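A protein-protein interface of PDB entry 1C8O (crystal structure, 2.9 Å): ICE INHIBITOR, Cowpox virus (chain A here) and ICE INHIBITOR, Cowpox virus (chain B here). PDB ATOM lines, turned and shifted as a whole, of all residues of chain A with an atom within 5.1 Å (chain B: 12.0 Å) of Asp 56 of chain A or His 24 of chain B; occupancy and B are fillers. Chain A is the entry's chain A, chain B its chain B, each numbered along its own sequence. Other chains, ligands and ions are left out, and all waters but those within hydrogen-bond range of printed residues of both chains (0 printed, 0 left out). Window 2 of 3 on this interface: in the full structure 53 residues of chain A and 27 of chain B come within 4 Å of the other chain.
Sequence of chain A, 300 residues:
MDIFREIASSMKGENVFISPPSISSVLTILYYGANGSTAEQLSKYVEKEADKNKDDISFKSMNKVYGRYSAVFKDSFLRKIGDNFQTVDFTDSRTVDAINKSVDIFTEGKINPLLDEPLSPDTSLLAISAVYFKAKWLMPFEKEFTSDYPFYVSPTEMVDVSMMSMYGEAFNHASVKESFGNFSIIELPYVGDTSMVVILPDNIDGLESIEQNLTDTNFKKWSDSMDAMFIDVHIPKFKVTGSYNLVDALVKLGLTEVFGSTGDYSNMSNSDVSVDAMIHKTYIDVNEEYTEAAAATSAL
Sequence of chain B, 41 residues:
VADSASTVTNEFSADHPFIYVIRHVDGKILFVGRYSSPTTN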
ATOM      1  N   LYS A  54     -31.145  25.005   4.513  1.00  0.00           N
ATOM      2  CA  LYS A  54     -31.087  24.344   5.811  1.00  0.00           C
ATOM      3  C   LYS A  54     -29.842  23.491   6.080  1.00  0.00           C
ATOM      4  O   LYS A  54     -28.783  23.695   5.479  1.00  0.00           O
ATOM      5  CB  LYS A  54     -32.352  23.499   6.008  1.00  0.00           C
ATOM      6  N   ASP A  55     -29.999  22.548   7.011  1.00  0.00           N
ATOM      7  CA  ASP A  55     -28.948  21.618   7.423  1.00  0.00           C
ATOM      8  C   ASP A  55     -29.494  20.648   8.483  1.00  0.00           C
ATOM      9  O   ASP A  55     -30.225  21.060   9.387  1.00  0.00           O
ATOM     10  CB  ASP A  55     -27.745  22.393   7.985  1.00  0.00           C
ATOM     11  N   ASP A  56     -29.162  19.362   8.361  1.00  0.00           N
ATOM     12  CA  ASP A  56     -29.610  18.358   9.335  1.00  0.00           C
ATOM     13  C   ASP A  56     -28.512  17.359   9.681  1.00  0.00           C
ATOM     14  O   ASP A  56     -28.518  16.219   9.212  1.00  0.00           O
ATOM     15  CB  ASP A  56     -30.847  17.594   8.836  1.00  0.00           C
ATOM     16  CG  ASP A  56     -30.553  16.714   7.633  1.00  0.00           C
ATOM     17  OD1 ASP A  56     -30.246  17.278   6.558  1.00  0.00           O
ATOM     18  OD2 ASP A  56     -30.629  15.467   7.763  1.00  0.00           O
ATOM     19  N   ILE A  57     -27.574  17.812  10.510  1.00  0.00           N
ATOM     20  CA  ILE A  57     -26.445  17.005  10.965  1.00  0.00           C
ATOM     21  C   ILE A  57     -25.229  17.050  10.031  1.00  0.00           C
ATOM     22  O   ILE A  57     -24.201  17.636  10.377  1.00  0.00           O
ATOM     23  CB  ILE A  57     -26.889  15.547  11.202  1.00  0.00           C
ATOM     24  N   SER A  58     -25.334  16.445   8.852  1.00  0.00           N
ATOM     25  CA  SER A  58     -24.201  16.441   7.941  1.00  0.00           C
ATOM     26  C   SER A  58     -24.548  16.835   6.520  1.00  0.00           C
ATOM     27  O   SER A  58     -23.732  16.702   5.607  1.00  0.00           O
ATOM     28  CB  SER A  58     -23.539  15.068   7.953  1.00  0.00           C
ATOM     29  OG  SER A  58     -23.040  14.778   9.247  1.00  0.00           O
ATOM     30  N   PHE A  59     -25.760  17.334   6.338  1.00  0.00           N
ATOM     31  CA  PHE A  59     -26.209  17.761   5.027  1.00  0.00           C
ATOM     32  C   PHE A  59     -26.629  19.217   5.109  1.00  0.00           C
ATOM     33  O   PHE A  59     -27.462  19.572   5.944  1.00  0.00           O
ATOM     34  CB  PHE A  59     -27.386  16.896   4.586  1.00  0.00           C
ATOM     35  CG  PHE A  59     -27.950  17.265   3.249  1.00  0.00           C
ATOM     36  CD1 PHE A  59     -29.059  18.087   3.152  1.00  0.00           C
ATOM     37  CD2 PHE A  59     -27.394  16.757   2.085  1.00  0.00           C
ATOM     38  CE1 PHE A  59     -29.612  18.392   1.918  1.00  0.00           C
ATOM     39  CE2 PHE A  59     -27.942  17.057   0.847  1.00  0.00           C
ATOM     40  CZ  PHE A  59     -29.052  17.875   0.767  1.00  0.00           C
ATOM     41  N   ASP A 193     -28.059  10.922  11.469  1.00  0.00           N
ATOM     42  CA  ASP A 193     -29.426  10.544  11.178  1.00  0.00           C
ATOM     43  C   ASP A 193     -29.579  10.171   9.717  1.00  0.00           C
ATOM     44  O   ASP A 193     -30.679  10.127   9.189  1.00  0.00           O
ATOM     45  CB  ASP A 193     -30.377  11.691  11.545  1.00  0.00           C
ATOM     46  CG  ASP A 193     -29.874  13.067  11.081  1.00  0.00           C
ATOM     47  OD1 ASP A 193     -30.608  14.061  11.302  1.00  0.00           O
ATOM     48  OD2 ASP A 193     -28.758  13.171  10.508  1.00  0.00           O
ATOM     49  N   THR A 194     -28.462   9.895   9.064  1.00  0.00           N
ATOM     50  CA  THR A 194     -28.495   9.527   7.667  1.00  0.00           C
ATOM     51  C   THR A 194     -27.808   8.182   7.467  1.00  0.00           C
ATOM     52  O   THR A 194     -26.957   7.781   8.269  1.00  0.00           O
ATOM     53  CB  THR A 194     -27.794  10.589   6.806  1.00  0.00           C
ATOM     54  OG1 THR A 194     -26.538  10.921   7.409  1.00  0.00           O
ATOM     55  CG2 THR A 194     -28.651  11.827   6.688  1.00  0.00           C
ATOM     56  N   SER A 195     -28.173   7.492   6.390  1.00  0.00           N
ATOM     57  CA  SER A 195     -27.591   6.193   6.092  1.00  0.00           C
ATOM     58  C   SER A 195     -27.500   5.968   4.593  1.00  0.00           C
ATOM     59  O   SER A 195     -28.041   6.739   3.802  1.00  0.00           O
ATOM     60  CB  SER A 195     -28.452   5.082   6.691  1.00  0.00           C
ATOM     61  OG  SER A 195     -29.705   5.007   6.020  1.00  0.00           O
ATOM     62  N   TYR B  20     -27.214   2.808  -5.004  1.00  0.00           N
ATOM     63  CA  TYR B  20     -26.984   3.226  -3.627  1.00  0.00           C
ATOM     64  C   TYR B  20     -27.774   4.498  -3.398  1.00  0.00           C
ATOM     65  O   TYR B  20     -27.972   5.279  -4.323  1.00  0.00           O
ATOM     66  CB  TYR B  20     -25.491   3.452  -3.318  1.00  0.00           C
ATOM     67  CG  TYR B  20     -24.754   4.461  -4.184  1.00  0.00           C
ATOM     68  CD1 TYR B  20     -24.169   5.601  -3.629  1.00  0.00           C
ATOM     69  CD2 TYR B  20     -24.583   4.240  -5.542  1.00  0.00           C
ATOM     70  CE1 TYR B  20     -23.426   6.493  -4.414  1.00  0.00           C
ATOM     71  CE2 TYR B  20     -23.850   5.116  -6.327  1.00  0.00           C
ATOM     72  CZ  TYR B  20     -23.271   6.242  -5.763  1.00  0.00           C
ATOM     73  OH  TYR B  20     -22.547   7.096  -6.575  1.00  0.00           O
ATOM     74  N   VAL B  21     -28.236   4.692  -2.170  1.00  0.00           N
ATOM     75  CA  VAL B  21     -29.038   5.860  -1.843  1.00  0.00           C
ATOM     76  C   VAL B  21     -28.692   6.412  -0.480  1.00  0.00           C
ATOM     77  O   VAL B  21     -28.698   5.679   0.499  1.00  0.00           O
ATOM     78  CB  VAL B  21     -30.527   5.516  -1.821  1.00  0.00           C
ATOM     79  CG1 VAL B  21     -31.311   6.697  -1.277  1.00  0.00           C
ATOM     80  CG2 VAL B  21     -30.999   5.125  -3.221  1.00  0.00           C
ATOM     81  N   ILE B  22     -28.379   7.697  -0.409  1.00  0.00           N
ATOM     82  CA  ILE B  22     -28.079   8.301   0.868  1.00  0.00           C
ATOM     83  C   ILE B  22     -29.395   8.916   1.292  1.00  0.00           C
ATOM     84  O   ILE B  22     -30.168   9.350   0.451  1.00  0.00           O
ATOM     85  CB  ILE B  22     -26.997   9.345   0.729  1.00  0.00           C
ATOM     86  CG1 ILE B  22     -25.729   8.669   0.221  1.00  0.00           C
ATOM     87  CG2 ILE B  22     -26.732  10.008   2.069  1.00  0.00           C
ATOM     88  CD1 ILE B  22     -24.568   9.608   0.014  1.00  0.00           C
ATOM     89  N   ARG B  23     -29.672   8.926   2.588  1.00  0.00           N
ATOM     90  CA  ARG B  23     -30.946   9.453   3.053  1.00  0.00           C
ATOM     91  C   ARG B  23     -30.951   9.772   4.541  1.00  0.00           C
ATOM     92  O   ARG B  23     -30.049   9.387   5.286  1.00  0.00           O
ATOM     93  CB  ARG B  23     -32.044   8.421   2.803  1.00  0.00           C
ATOM     94  CG  ARG B  23     -31.904   7.229   3.736  1.00  0.00           C
ATOM     95  CD  ARG B  23     -32.592   6.003   3.205  1.00  0.00           C
ATOM     96  NE  ARG B  23     -34.053   6.062   3.284  1.00  0.00           N
ATOM     97  CZ  ARG B  23     -34.784   5.373   4.156  1.00  0.00           C
ATOM     98  NH1 ARG B  23     -34.193   4.564   5.044  1.00  0.00           N
ATOM     99  NH2 ARG B  23     -36.107   5.482   4.121  1.00  0.00           N
ATOM    100  N   HIS B  24     -32.004  10.474   4.950  1.00  0.00           N
ATOM    101  CA  HIS B  24     -32.230  10.835   6.338  1.00  0.00           C
ATOM    102  C   HIS B  24     -32.908   9.584   6.880  1.00  0.00           C
ATOM    103  O   HIS B  24     -33.812   9.053   6.240  1.00  0.00           O
ATOM    104  CB  HIS B  24     -33.187  12.025   6.416  1.00  0.00           C
ATOM    105  CG  HIS B  24     -33.521  12.449   7.815  1.00  0.00           C
ATOM    106  ND1 HIS B  24     -34.744  12.992   8.156  1.00  0.00           N
ATOM    107  CD2 HIS B  24     -32.790  12.423   8.957  1.00  0.00           C
ATOM    108  CE1 HIS B  24     -34.752  13.281   9.447  1.00  0.00           C
ATOM    109  NE2 HIS B  24     -33.579  12.946   9.956  1.00  0.00           N
ATOM    110  N   VAL B  25     -32.454   9.105   8.033  1.00  0.00           N
ATOM    111  CA  VAL B  25     -33.011   7.910   8.651  1.00  0.00           C
ATOM    112  C   VAL B  25     -34.360   7.540   8.053  1.00  0.00           C
ATOM    113  O   VAL B  25     -34.463   6.597   7.267  1.00  0.00           O
ATOM    114  CB  VAL B  25     -33.182   8.093  10.173  1.00  0.00           C
ATOM    115  CG1 VAL B  25     -31.818   8.060  10.863  1.00  0.00           C
ATOM    116  CG2 VAL B  25     -33.906   9.416  10.468  1.00  0.00           C
ATOM    117  N   ASP B  26     -35.396   8.286   8.410  1.00  0.00           N
ATOM    118  CA  ASP B  26     -36.728   8.006   7.892  1.00  0.00           C
ATOM    119  C   ASP B  26     -37.226   9.204   7.099  1.00  0.00           C
ATOM    120  O   ASP B  26     -38.433   9.446   7.000  1.00  0.00           O
ATOM    121  CB  ASP B  26     -37.684   7.702   9.047  1.00  0.00           C
ATOM    122  N   GLY B  27     -36.284   9.946   6.523  1.00  0.00           N
ATOM    123  CA  GLY B  27     -36.630  11.138   5.769  1.00  0.00           C
ATOM    124  C   GLY B  27     -36.474  11.041   4.269  1.00  0.00           C
ATOM    125  O   GLY B  27     -36.512   9.960   3.694  1.00  0.00           O
ATOM    126  N   LYS B  28     -36.299  12.194   3.641  1.00  0.00           N
ATOM    127  CA  LYS B  28     -36.152  12.268   2.197  1.00  0.00           C
ATOM    128  C   LYS B  28     -34.844  11.655   1.700  1.00  0.00           C
ATOM    129  O   LYS B  28     -33.907  11.439   2.467  1.00  0.00           O
ATOM    130  CB  LYS B  28     -36.251  13.733   1.740  1.00  0.00           C
ATOM    131  N   ILE B  29     -34.797  11.373   0.405  1.00  0.00           N
ATOM    132  CA  ILE B  29     -33.601  10.827  -0.218  1.00  0.00           C
ATOM    133  C   ILE B  29     -32.669  11.996  -0.524  1.00  0.00           C
ATOM    134  O   ILE B  29     -33.026  12.897  -1.269  1.00  0.00           O
ATOM    135  CB  ILE B  29     -33.929  10.122  -1.545  1.00  0.00           C
ATOM    136  CG1 ILE B  29     -34.656   8.812  -1.270  1.00  0.00           C
ATOM    137  CG2 ILE B  29     -32.660   9.905  -2.348  1.00  0.00           C
ATOM    138  CD1 ILE B  29     -36.050   9.002  -0.720  1.00  0.00           C
ATOM    139  N   LEU B  30     -31.480  11.985   0.056  1.00  0.00           N
ATOM    140  CA  LEU B  30     -30.533  13.048  -0.190  1.00  0.00           C
ATOM    141  C   LEU B  30     -29.812  12.878  -1.518  1.00  0.00           C
ATOM    142  O   LEU B  30     -29.552  13.849  -2.220  1.00  0.00           O
ATOM    143  CB  LEU B  30     -29.524  13.122   0.948  1.00  0.00           C
ATOM    144  CG  LEU B  30     -29.944  14.089   2.054  1.00  0.00           C
ATOM    145  CD1 LEU B  30     -31.458  14.117   2.198  1.00  0.00           C
ATOM    146  CD2 LEU B  30     -29.254  13.694   3.343  1.00  0.00           C
ATOM    147  N   PHE B  31     -29.495  11.642  -1.865  1.00  0.00           N
ATOM    148  CA  PHE B  31     -28.811  11.361  -3.108  1.00  0.00           C
ATOM    149  C   PHE B  31     -29.268  10.006  -3.617  1.00  0.00           C
ATOM    150  O   PHE B  31     -30.042   9.321  -2.968  1.00  0.00           O
ATOM    151  CB  PHE B  31     -27.312  11.328  -2.871  1.00  0.00           C
ATOM    152  CG  PHE B  31     -26.748  12.622  -2.393  1.00  0.00           C
ATOM    153  CD1 PHE B  31     -26.448  13.632  -3.291  1.00  0.00           C
ATOM    154  CD2 PHE B  31     -26.493  12.825  -1.042  1.00  0.00           C
ATOM    155  CE1 PHE B  31     -25.897  14.821  -2.857  1.00  0.00           C
ATOM    156  CE2 PHE B  31     -25.943  14.011  -0.594  1.00  0.00           C
ATOM    157  CZ  PHE B  31     -25.642  15.010  -1.502  1.00  0.00           C
ATOM    158  N   VAL B  32     -28.775   9.618  -4.780  1.00  0.00           N
ATOM    159  CA  VAL B  32     -29.120   8.343  -5.375  1.00  0.00           C
ATOM    160  C   VAL B  32     -28.355   8.185  -6.679  1.00  0.00           C
ATOM    161  O   VAL B  32     -28.467   9.016  -7.583  1.00  0.00           O
ATOM    162  CB  VAL B  32     -30.637   8.225  -5.641  1.00  0.00           C
ATOM    163  CG1 VAL B  32     -31.164   9.493  -6.239  1.00  0.00           C
ATOM    164  CG2 VAL B  32     -30.904   7.041  -6.564  1.00  0.00           C
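The backbone NH (N) of Ser 195 of chain A is in hydrogen-bond range of the backbone carbonyl oxygen (O) of Arg 23 of chain B, 2.9 Å away.
OD1 of Asp 193 of chain A lies within hydrogen-bond range of NE2 of His 24 of chain B (3.4 Å).
The backbone carbonyl oxygen (O) of Asp 193 of chain A sits close to the backbone NH (N) of Val 25 of chain B, 2.4 Å away.
O of Val 25 of chain B is in hydrogen-bond range of NH1 of Arg 23 of chain B (3.0 Å).
N of Phe 31 of chain B sits at hydrogen-bond distance from O of Ile 22 of chain B, 3.3 Å away.
The backbone NH (N) of Leu 30 of chain B lies within hydrogen-bond range of the backbone carbonyl oxygen (O) of Ile 22 of chain B (3.0 Å).
Among the printed residues, pairs that only touch across the chains: Thr 194 of chain A with Arg 23 of chain B, Ser 195 of chain A with Ile 22 of chain B, Ser 195 of chain A with Val 21 of chain B, Phe 59 of chain A with Leu 30 of chain B, Thr 194 of chain A with His 24 of chain B, Phe 59 of chain A with Phe 31 of chain B, Thr 194 of chain A with Leu 30 of chain B, Asp 56 of chain A with His 24 of chain B and Thr 194 of chain A with Val 25 of chain B.
No residue of chain B comes within 4 Å of Lys 54 of chain A.
No residue of chain B comes within 4 Å of Asp 55 of chain A.
Asp 193 of chain A touches two residues of chain B.
Of chain A, only Asp 56 (3.9 Å), Asp 193 (3.1 Å) and Thr 194 (3.7 Å) come within 4 Å of His 24 of chain B.
Ile 29 of chain B touches none of the printed residues of chain A.
Of the printed residues of chain A, Leu 30 of chain B touches Phe 59 and Thr 194.
Of the printed residues of chain A, Phe 31 of chain B touches Phe 59 (3.9 Å).
The nearest printed residue of chain A that does not touch His 24 of chain B is Ser 195 of chain A (5.1 Å).
The nearest printed residue of chain A that does not touch Arg 23 of chain B is Asp 193 of chain A (4.02 Å).
Hydrophobic or aromatic side chains of chain A that line the printed part of chain B: Phe 59.
Hydrophobic or aromatic side chains of chain B that line the printed part of chain A: Ile 22, His 24, Val 25, Leu 30 and Phe 31.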
